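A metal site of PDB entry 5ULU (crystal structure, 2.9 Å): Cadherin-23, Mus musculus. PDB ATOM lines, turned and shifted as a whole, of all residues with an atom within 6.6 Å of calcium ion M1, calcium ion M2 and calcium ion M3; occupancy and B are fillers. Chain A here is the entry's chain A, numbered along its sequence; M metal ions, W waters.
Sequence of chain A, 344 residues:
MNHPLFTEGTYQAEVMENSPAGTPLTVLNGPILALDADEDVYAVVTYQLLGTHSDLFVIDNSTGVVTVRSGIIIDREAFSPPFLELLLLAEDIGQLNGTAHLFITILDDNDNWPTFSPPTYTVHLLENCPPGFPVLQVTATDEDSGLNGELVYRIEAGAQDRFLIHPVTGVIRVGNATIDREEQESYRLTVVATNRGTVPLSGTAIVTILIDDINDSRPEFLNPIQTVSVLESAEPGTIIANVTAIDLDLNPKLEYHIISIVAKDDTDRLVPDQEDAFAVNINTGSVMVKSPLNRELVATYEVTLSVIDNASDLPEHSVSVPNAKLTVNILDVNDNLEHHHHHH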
ATOM      1  N   GLU A 127      -0.240  10.491 -30.623  1.00  0.00           N
ATOM      2  CA  GLU A 127       0.934  11.317 -30.949  1.00  0.00           C
ATOM      3  C   GLU A 127       2.265  10.556 -30.819  1.00  0.00           C
ATOM      4  O   GLU A 127       2.310   9.391 -30.373  1.00  0.00           O
ATOM      5  CB  GLU A 127       0.958  12.623 -30.119  1.00  0.00           C
ATOM      6  CG  GLU A 127       1.109  12.458 -28.610  1.00  0.00           C
ATOM      7  CD  GLU A 127       1.413  13.774 -27.886  1.00  0.00           C
ATOM      8  OE1 GLU A 127       0.829  14.021 -26.821  1.00  0.00           O
ATOM      9  OE2 GLU A 127       2.231  14.585 -28.369  1.00  0.00           O
ATOM     10  N   ASN A 128       3.334  11.213 -31.278  1.00  0.00           N
ATOM     11  CA  ASN A 128       4.707  10.658 -31.242  1.00  0.00           C
ATOM     12  C   ASN A 128       4.869   9.361 -32.000  1.00  0.00           C
ATOM     13  O   ASN A 128       5.805   8.592 -31.737  1.00  0.00           O
ATOM     14  CB  ASN A 128       5.171  10.439 -29.804  1.00  0.00           C
ATOM     15  CG  ASN A 128       4.970  11.643 -28.933  1.00  0.00           C
ATOM     16  OD1 ASN A 128       4.914  12.797 -29.396  1.00  0.00           O
ATOM     17  ND2 ASN A 128       4.875  11.377 -27.639  1.00  0.00           N
ATOM     18  N   ILE A 179       4.797  14.180 -35.101  1.00  0.00           N
ATOM     19  CA  ILE A 179       3.458  14.692 -34.948  1.00  0.00           C
ATOM     20  C   ILE A 179       3.188  14.796 -33.435  1.00  0.00           C
ATOM     21  O   ILE A 179       2.944  13.815 -32.723  1.00  0.00           O
ATOM     22  CB  ILE A 179       2.423  13.913 -35.811  1.00  0.00           C
ATOM     23  CG1 ILE A 179       2.206  12.489 -35.324  1.00  0.00           C
ATOM     24  CG2 ILE A 179       2.840  13.903 -37.283  1.00  0.00           C
ATOM     25  CD1 ILE A 179       0.911  12.336 -34.535  1.00  0.00           C
ATOM     26  N   ASP A 180       3.357  16.018 -32.958  1.00  0.00           N
ATOM     27  CA  ASP A 180       3.198  16.369 -31.548  1.00  0.00           C
ATOM     28  C   ASP A 180       1.817  16.977 -31.367  1.00  0.00           C
ATOM     29  O   ASP A 180       1.459  17.932 -32.078  1.00  0.00           O
ATOM     30  CB  ASP A 180       4.270  17.397 -31.195  1.00  0.00           C
ATOM     31  CG  ASP A 180       4.289  17.767 -29.738  1.00  0.00           C
ATOM     32  OD1 ASP A 180       3.726  17.016 -28.915  1.00  0.00           O
ATOM     33  OD2 ASP A 180       4.913  18.809 -29.408  1.00  0.00           O
ATOM     34  N   ARG A 181       1.017  16.445 -30.435  1.00  0.00           N
ATOM     35  CA  ARG A 181      -0.290  17.048 -30.169  1.00  0.00           C
ATOM     36  C   ARG A 181      -0.163  18.518 -29.690  1.00  0.00           C
ATOM     37  O   ARG A 181      -0.935  19.381 -30.095  1.00  0.00           O
ATOM     38  CB  ARG A 181      -1.094  16.227 -29.166  1.00  0.00           C
ATOM     39  CG  ARG A 181      -2.614  16.475 -29.277  1.00  0.00           C
ATOM     40  CD  ARG A 181      -3.349  15.988 -28.054  1.00  0.00           C
ATOM     41  NE  ARG A 181      -2.936  16.780 -26.903  1.00  0.00           N
ATOM     42  CZ  ARG A 181      -3.387  17.997 -26.626  1.00  0.00           C
ATOM     43  NH1 ARG A 181      -4.314  18.566 -27.380  1.00  0.00           N
ATOM     44  NH2 ARG A 181      -2.892  18.640 -25.573  1.00  0.00           N
ATOM     45  N   GLU A 182       0.852  18.793 -28.875  1.00  0.00           N
ATOM     46  CA  GLU A 182       1.045  20.115 -28.310  1.00  0.00           C
ATOM     47  C   GLU A 182       1.568  21.132 -29.342  1.00  0.00           C
ATOM     48  O   GLU A 182       1.606  22.338 -29.055  1.00  0.00           O
ATOM     49  CB  GLU A 182       1.987  20.058 -27.102  1.00  0.00           C
ATOM     50  CG  GLU A 182       1.426  19.395 -25.851  1.00  0.00           C
ATOM     51  CD  GLU A 182       1.248  17.888 -25.958  1.00  0.00           C
ATOM     52  OE1 GLU A 182       0.335  17.344 -25.326  1.00  0.00           O
ATOM     53  OE2 GLU A 182       2.012  17.204 -26.667  1.00  0.00           O
ATOM     54  N   GLU A 183       1.982  20.651 -30.510  1.00  0.00           N
ATOM     55  CA  GLU A 183       2.325  21.498 -31.681  1.00  0.00           C
ATOM     56  C   GLU A 183       1.076  21.832 -32.475  1.00  0.00           C
ATOM     57  O   GLU A 183       0.869  22.964 -32.867  1.00  0.00           O
ATOM     58  CB  GLU A 183       3.344  20.761 -32.577  1.00  0.00           C
ATOM     59  CG  GLU A 183       3.685  21.334 -33.952  1.00  0.00           C
ATOM     60  CD  GLU A 183       4.468  20.310 -34.787  1.00  0.00           C
ATOM     61  OE1 GLU A 183       5.666  20.574 -35.054  1.00  0.00           O
ATOM     62  OE2 GLU A 183       3.891  19.229 -35.125  1.00  0.00           O
ATOM     63  N   ASP A 212      -4.795  12.271 -30.717  1.00  0.00           N
ATOM     64  CA  ASP A 212      -4.994  11.876 -29.323  1.00  0.00           C
ATOM     65  C   ASP A 212      -3.761  12.185 -28.501  1.00  0.00           C
ATOM     66  O   ASP A 212      -2.674  12.333 -29.040  1.00  0.00           O
ATOM     67  CB  ASP A 212      -5.382  10.403 -29.227  1.00  0.00           C
ATOM     68  CG  ASP A 212      -6.771  10.116 -29.758  1.00  0.00           C
ATOM     69  OD1 ASP A 212      -7.435  11.051 -30.294  1.00  0.00           O
ATOM     70  OD2 ASP A 212      -7.223   8.961 -29.633  1.00  0.00           O
ATOM     71  N   ASP A 213      -3.936  12.271 -27.191  1.00  0.00           N
ATOM     72  CA  ASP A 213      -2.896  12.767 -26.314  1.00  0.00           C
ATOM     73  C   ASP A 213      -2.122  11.659 -25.629  1.00  0.00           C
ATOM     74  O   ASP A 213      -2.677  10.645 -25.210  1.00  0.00           O
ATOM     75  CB  ASP A 213      -3.500  13.665 -25.225  1.00  0.00           C
ATOM     76  CG  ASP A 213      -2.438  14.387 -24.395  1.00  0.00           C
ATOM     77  OD1 ASP A 213      -1.583  15.061 -25.009  1.00  0.00           O
ATOM     78  OD2 ASP A 213      -2.466  14.269 -23.130  1.00  0.00           O
ATOM     79  N   ILE A 214      -0.818  11.893 -25.546  1.00  0.00           N
ATOM     80  CA  ILE A 214       0.043  11.238 -24.593  1.00  0.00           C
ATOM     81  C   ILE A 214       0.484  12.352 -23.647  1.00  0.00           C
ATOM     82  O   ILE A 214       0.819  13.455 -24.111  1.00  0.00           O
ATOM     83  CB  ILE A 214       1.268  10.610 -25.296  1.00  0.00           C
ATOM     84  CG1 ILE A 214       0.827   9.509 -26.269  1.00  0.00           C
ATOM     85  CG2 ILE A 214       2.223  10.003 -24.270  1.00  0.00           C
ATOM     86  CD1 ILE A 214       1.963   8.856 -27.022  1.00  0.00           C
ATOM     87  N   ASN A 215       0.473  12.071 -22.341  1.00  0.00           N
ATOM     88  CA  ASN A 215       1.034  13.008 -21.363  1.00  0.00           C
ATOM     89  C   ASN A 215       2.564  12.935 -21.452  1.00  0.00           C
ATOM     90  O   ASN A 215       3.255  12.178 -20.718  1.00  0.00           O
ATOM     91  CB  ASN A 215       0.506  12.729 -19.965  1.00  0.00           C
ATOM     92  CG  ASN A 215       0.923  13.789 -18.974  1.00  0.00           C
ATOM     93  OD1 ASN A 215       1.753  14.636 -19.279  1.00  0.00           O
ATOM     94  ND2 ASN A 215       0.363  13.734 -17.781  1.00  0.00           N
ATOM     95  N   ASP A 216       3.080  13.715 -22.391  1.00  0.00           N
ATOM     96  CA  ASP A 216       4.468  13.601 -22.821  1.00  0.00           C
ATOM     97  C   ASP A 216       5.237  14.899 -22.676  1.00  0.00           C
ATOM     98  O   ASP A 216       6.391  14.972 -23.091  1.00  0.00           O
ATOM     99  CB  ASP A 216       4.520  13.078 -24.275  1.00  0.00           C
ATOM    100  CG  ASP A 216       4.026  14.097 -25.306  1.00  0.00           C
ATOM    101  OD1 ASP A 216       3.389  15.103 -24.957  1.00  0.00           O
ATOM    102  OD2 ASP A 216       4.296  13.906 -26.516  1.00  0.00           O
ATOM    103  N   SER A 217       4.613  15.909 -22.049  1.00  0.00           N
ATOM    104  CA  SER A 217       5.256  17.212 -21.823  1.00  0.00           C
ATOM    105  C   SER A 217       5.712  17.432 -20.385  1.00  0.00           C
ATOM    106  O   SER A 217       5.200  16.826 -19.418  1.00  0.00           O
ATOM    107  CB  SER A 217       4.364  18.378 -22.233  1.00  0.00           C
ATOM    108  OG  SER A 217       4.269  18.379 -23.628  1.00  0.00           O
ATOM    109  N   ARG A 218       6.674  18.326 -20.285  1.00  0.00           N
ATOM    110  CA  ARG A 218       7.312  18.673 -19.047  1.00  0.00           C
ATOM    111  C   ARG A 218       6.516  19.822 -18.455  1.00  0.00           C
ATOM    112  O   ARG A 218       6.253  20.791 -19.156  1.00  0.00           O
ATOM    113  CB  ARG A 218       8.752  19.107 -19.352  1.00  0.00           C
ATOM    114  CG  ARG A 218       9.712  19.064 -18.193  1.00  0.00           C
ATOM    115  CD  ARG A 218      11.130  19.358 -18.657  1.00  0.00           C
ATOM    116  NE  ARG A 218      11.704  18.287 -19.483  1.00  0.00           N
ATOM    117  CZ  ARG A 218      12.060  17.078 -19.047  1.00  0.00           C
ATOM    118  NH1 ARG A 218      12.550  16.194 -19.921  1.00  0.00           N
ATOM    119  NH2 ARG A 218      11.944  16.715 -17.768  1.00  0.00           N
ATOM    120  N   PRO A 219       6.127  19.719 -17.166  1.00  0.00           N
ATOM    121  CA  PRO A 219       5.651  20.940 -16.534  1.00  0.00           C
ATOM    122  C   PRO A 219       6.773  21.927 -16.544  1.00  0.00           C
ATOM    123  O   PRO A 219       7.888  21.527 -16.297  1.00  0.00           O
ATOM    124  CB  PRO A 219       5.378  20.503 -15.098  1.00  0.00           C
ATOM    125  CG  PRO A 219       6.240  19.307 -14.889  1.00  0.00           C
ATOM    126  CD  PRO A 219       6.249  18.605 -16.206  1.00  0.00           C
ATOM    127  N   ASP A 247       1.621  22.738 -17.687  1.00  0.00           N
ATOM    128  CA  ASP A 247       1.924  21.513 -18.426  1.00  0.00           C
ATOM    129  C   ASP A 247       0.914  21.398 -19.541  1.00  0.00           C
ATOM    130  O   ASP A 247      -0.259  21.170 -19.300  1.00  0.00           O
ATOM    131  CB  ASP A 247       1.857  20.270 -17.512  1.00  0.00           C
ATOM    132  CG  ASP A 247       2.359  19.001 -18.213  1.00  0.00           C
ATOM    133  OD1 ASP A 247       3.437  19.033 -18.802  1.00  0.00           O
ATOM    134  OD2 ASP A 247       1.670  17.977 -18.191  1.00  0.00           O
ATOM    135  N   LEU A 248       1.395  21.493 -20.778  1.00  0.00           N
ATOM    136  CA  LEU A 248       0.564  21.611 -21.963  1.00  0.00           C
ATOM    137  C   LEU A 248      -0.189  20.357 -22.417  1.00  0.00           C
ATOM    138  O   LEU A 248      -0.873  20.385 -23.434  1.00  0.00           O
ATOM    139  CB  LEU A 248       1.390  22.168 -23.143  1.00  0.00           C
ATOM    140  CG  LEU A 248       1.845  23.648 -23.116  1.00  0.00           C
ATOM    141  CD1 LEU A 248       1.805  24.227 -24.526  1.00  0.00           C
ATOM    142  CD2 LEU A 248       0.998  24.541 -22.205  1.00  0.00           C
ATOM    143  N   ASP A 249      -0.112  19.272 -21.670  1.00  0.00           N
ATOM    144  CA  ASP A 249      -0.936  18.111 -21.974  1.00  0.00           C
ATOM    145  C   ASP A 249      -2.351  18.317 -21.450  1.00  0.00           C
ATOM    146  O   ASP A 249      -2.600  19.203 -20.623  1.00  0.00           O
ATOM    147  CB  ASP A 249      -0.334  16.864 -21.322  1.00  0.00           C
ATOM    148  CG  ASP A 249       1.101  16.588 -21.777  1.00  0.00           C
ATOM    149  OD1 ASP A 249       1.294  16.333 -23.001  1.00  0.00           O
ATOM    150  OD2 ASP A 249       2.025  16.617 -20.914  1.00  0.00           O
ATOM    151  N   LEU A 250      -3.253  17.480 -21.942  1.00  0.00           N
ATOM    152  CA  LEU A 250      -4.573  17.246 -21.313  1.00  0.00           C
ATOM    153  C   LEU A 250      -4.412  16.642 -19.900  1.00  0.00           C
ATOM    154  O   LEU A 250      -3.556  15.777 -19.671  1.00  0.00           O
ATOM    155  CB  LEU A 250      -5.396  16.271 -22.154  1.00  0.00           C
ATOM    156  CG  LEU A 250      -6.251  16.767 -23.324  1.00  0.00           C
ATOM    157  CD1 LEU A 250      -5.567  17.862 -24.128  1.00  0.00           C
ATOM    158  CD2 LEU A 250      -6.667  15.592 -24.216  1.00  0.00           C
ATOM    159  N   PRO A 252      -3.153  17.286 -16.812  1.00  0.00           N
ATOM    160  CA  PRO A 252      -1.976  17.200 -15.950  1.00  0.00           C
ATOM    161  C   PRO A 252      -2.416  17.360 -14.514  1.00  0.00           C
ATOM    162  O   PRO A 252      -3.435  17.995 -14.277  1.00  0.00           O
ATOM    163  CB  PRO A 252      -1.157  18.409 -16.364  1.00  0.00           C
ATOM    164  CG  PRO A 252      -2.167  19.420 -16.793  1.00  0.00           C
ATOM    165  CD  PRO A 252      -3.353  18.652 -17.307  1.00  0.00           C
ATOM    166  N   LEU A 254      -0.199  18.643 -11.354  1.00  0.00           N
ATOM    167  CA  LEU A 254       1.070  19.107 -10.854  1.00  0.00           C
ATOM    168  C   LEU A 254       1.089  19.114  -9.340  1.00  0.00           C
ATOM    169  O   LEU A 254       0.043  19.279  -8.701  1.00  0.00           O
ATOM    170  CB  LEU A 254       1.341  20.534 -11.335  1.00  0.00           C
ATOM    171  CG  LEU A 254       1.128  20.903 -12.814  1.00  0.00           C
ATOM    172  CD1 LEU A 254       1.667  22.301 -13.115  1.00  0.00           C
ATOM    173  CD2 LEU A 254       1.770  19.888 -13.730  1.00  0.00           C
ATOM    174  N   ASP A 309       4.380  16.791 -12.847  1.00  0.00           N
ATOM    175  CA  ASP A 309       3.104  16.361 -13.371  1.00  0.00           C
ATOM    176  C   ASP A 309       2.974  14.889 -13.032  1.00  0.00           C
ATOM    177  O   ASP A 309       3.707  14.069 -13.567  1.00  0.00           O
ATOM    178  CB  ASP A 309       3.038  16.590 -14.879  1.00  0.00           C
ATOM    179  CG  ASP A 309       1.852  15.889 -15.527  1.00  0.00           C
ATOM    180  OD1 ASP A 309       0.917  15.449 -14.807  1.00  0.00           O
ATOM    181  OD2 ASP A 309       1.887  15.752 -16.766  1.00  0.00           O
ATOM    182  N   ALA A 311       0.649  12.723 -13.652  1.00  0.00           N
ATOM    183  CA  ALA A 311      -0.088  11.873 -14.579  1.00  0.00           C
ATOM    184  C   ALA A 311       0.756  11.490 -15.809  1.00  0.00           C
ATOM    185  O   ALA A 311       0.227  10.969 -16.802  1.00  0.00           O
ATOM    186  CB  ALA A 311      -1.359  12.581 -14.992  1.00  0.00           C
ATOM    187  N   SER A 312       2.074  11.735 -15.742  1.00  0.00           N
ATOM    188  CA  SER A 312       2.908  11.732 -16.939  1.00  0.00           C
ATOM    189  C   SER A 312       3.184  10.302 -17.348  1.00  0.00           C
ATOM    190  O   SER A 312       3.496   9.455 -16.504  1.00  0.00           O
ATOM    191  CB  SER A 312       4.199  12.539 -16.736  1.00  0.00           C
ATOM    192  OG  SER A 312       4.710  13.033 -17.971  1.00  0.00           O
ATOM    193  N   ASP A 313       3.030  10.035 -18.634  1.00  0.00           N
ATOM    194  CA  ASP A 313       3.208   8.685 -19.209  1.00  0.00           C
ATOM    195  C   ASP A 313       4.673   8.361 -19.453  1.00  0.00           C
ATOM    196  O   ASP A 313       4.999   7.220 -19.711  1.00  0.00           O
ATOM    197  CB  ASP A 313       2.453   8.587 -20.539  1.00  0.00           C
ATOM    198  CG  ASP A 313       0.952   8.794 -20.376  1.00  0.00           C
ATOM    199  OD1 ASP A 313       0.364   8.107 -19.502  1.00  0.00           O
ATOM    200  OD2 ASP A 313       0.364   9.618 -21.120  1.00  0.00           O
ATOM    201  N   HIS A 317       9.907  12.829 -19.029  1.00  0.00           N
ATOM    202  CA  HIS A 317       9.300  14.156 -19.239  1.00  0.00           C
ATOM    203  C   HIS A 317       8.413  14.665 -18.088  1.00  0.00           C
ATOM    204  O   HIS A 317       7.656  15.603 -18.276  1.00  0.00           O
ATOM    205  CB  HIS A 317       8.493  14.143 -20.556  1.00  0.00           C
ATOM    206  CG  HIS A 317       9.352  14.118 -21.778  1.00  0.00           C
ATOM    207  ND1 HIS A 317      10.504  14.862 -21.887  1.00  0.00           N
ATOM    208  CD2 HIS A 317       9.208  13.469 -22.945  1.00  0.00           C
ATOM    209  CE1 HIS A 317      11.047  14.656 -23.074  1.00  0.00           C
ATOM    210  NE2 HIS A 317      10.274  13.818 -23.734  1.00  0.00           N
ATOM    211  N   SER A 318       8.536  14.086 -16.909  1.00  0.00           N
ATOM    212  CA  SER A 318       7.537  14.313 -15.877  1.00  0.00           C
ATOM    213  C   SER A 318       7.931  15.351 -14.823  1.00  0.00           C
ATOM    214  O   SER A 318       7.224  15.474 -13.842  1.00  0.00           O
ATOM    215  CB  SER A 318       7.176  12.997 -15.198  1.00  0.00           C
ATOM    216  OG  SER A 318       8.080  12.696 -14.161  1.00  0.00           O
HETATM  217 CA    CA M   1       3.980  16.006 -27.240  1.00  0.00          CA
HETATM  218 CA    CA M   2       0.795  15.376 -25.028  1.00  0.00          CA
HETATM  219 CA    CA M   3       3.005  16.263 -18.569  1.00  0.00          CA
HETATM  220  O   HOH W   1       6.594  15.659 -29.196  1.00  0.00           O
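Asn 128 touches calcium ion M1. Of the 27 residues printed, 5 come within 4 Å of calcium ion M1. The nearest printed residue that does not touch calcium ion M1 is Ser 217 (4.3 Å).
OE1 of Glu 182 lies close to NH2 of Arg 181 (3.5 Å). The backbone carbonyl oxygen (O) of Asn 215 sits at hydrogen-bond distance from the side-chain hydroxyl (OG) of Ser 312. The backbone NH of Asn 215 is in hydrogen-bond range of the side-chain carboxylate of Asp 313 (2.7 Å). N of Ala 311 lies within hydrogen-bond range of OD1 of Asp 309 (3.0 Å). The side-chain amide nitrogen (ND2) of Asn 128 sits close to the side-chain carboxylate (OD2) of Asp 216 (2.8 Å). The side-chain carboxylate (OE2) of Glu 127 lies close to the side-chain amide oxygen (OD1) of Asn 128. The side-chain carboxylate (OE2) of Glu 127 sits close to the backbone NH (N) of Arg 181 (3.0 Å). The side-chain carboxylate (OD1) of Asp 213 lies close to the guanidinium group (NE) of Arg 181, 2.9 Å away.
Calcium ion M2 is bound by the side-chain carboxylate (OE1) of Glu 182 (2.0 Å), the backbone carbonyl oxygen (O) of Ile 214 (2.1 Å), the side-chain carboxylate (OE1) of Glu 127 (2.2 Å), the side-chain carboxylate (OD1) of Asp 249 (2.3 Å), the side-chain carboxylate (OD1) of Asp 213 (2.4 Å), the side-chain carboxylate (OD1) of Asp 216 (2.6 Å) and the side-chain carboxylate (OE2) of Glu 182 (2.7 Å). Calcium ion M2 has seven donor atoms within binding distance.
Six residues have an atom within 4 Å of calcium ion M2: Glu 127, Glu 182, Asp 213, Ile 214, Asp 216 and Asp 249.
Calcium ion M1 is bound by OD1 of Asp 180 (2.0 Å), OD2 of Asp 216 (2.2 Å), OE2 of Glu 182 (2.4 Å), OE2 of Glu 127 (2.5 Å) and OD1 of Asp 216 (2.5 Å).
OG of Ser 312 touches calcium ion M3 (3.7 Å). Of the 27 residues printed, 6 come within 4 Å of calcium ion M3. The nearest printed residue that does not touch calcium ion M3 is Arg 218 (4.5 Å).
Calcium ion M3 is bound by the side-chain amide oxygen (OD1) of Asn 215, the side-chain carboxylate (OD2) of Asp 309, the side-chain carboxylate (OD2) of Asp 247, the backbone carbonyl oxygen (O) of Ser 217, the side-chain carboxylate (OD2) of Asp 249 and the side-chain carboxylate (OD1) of Asp 247.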
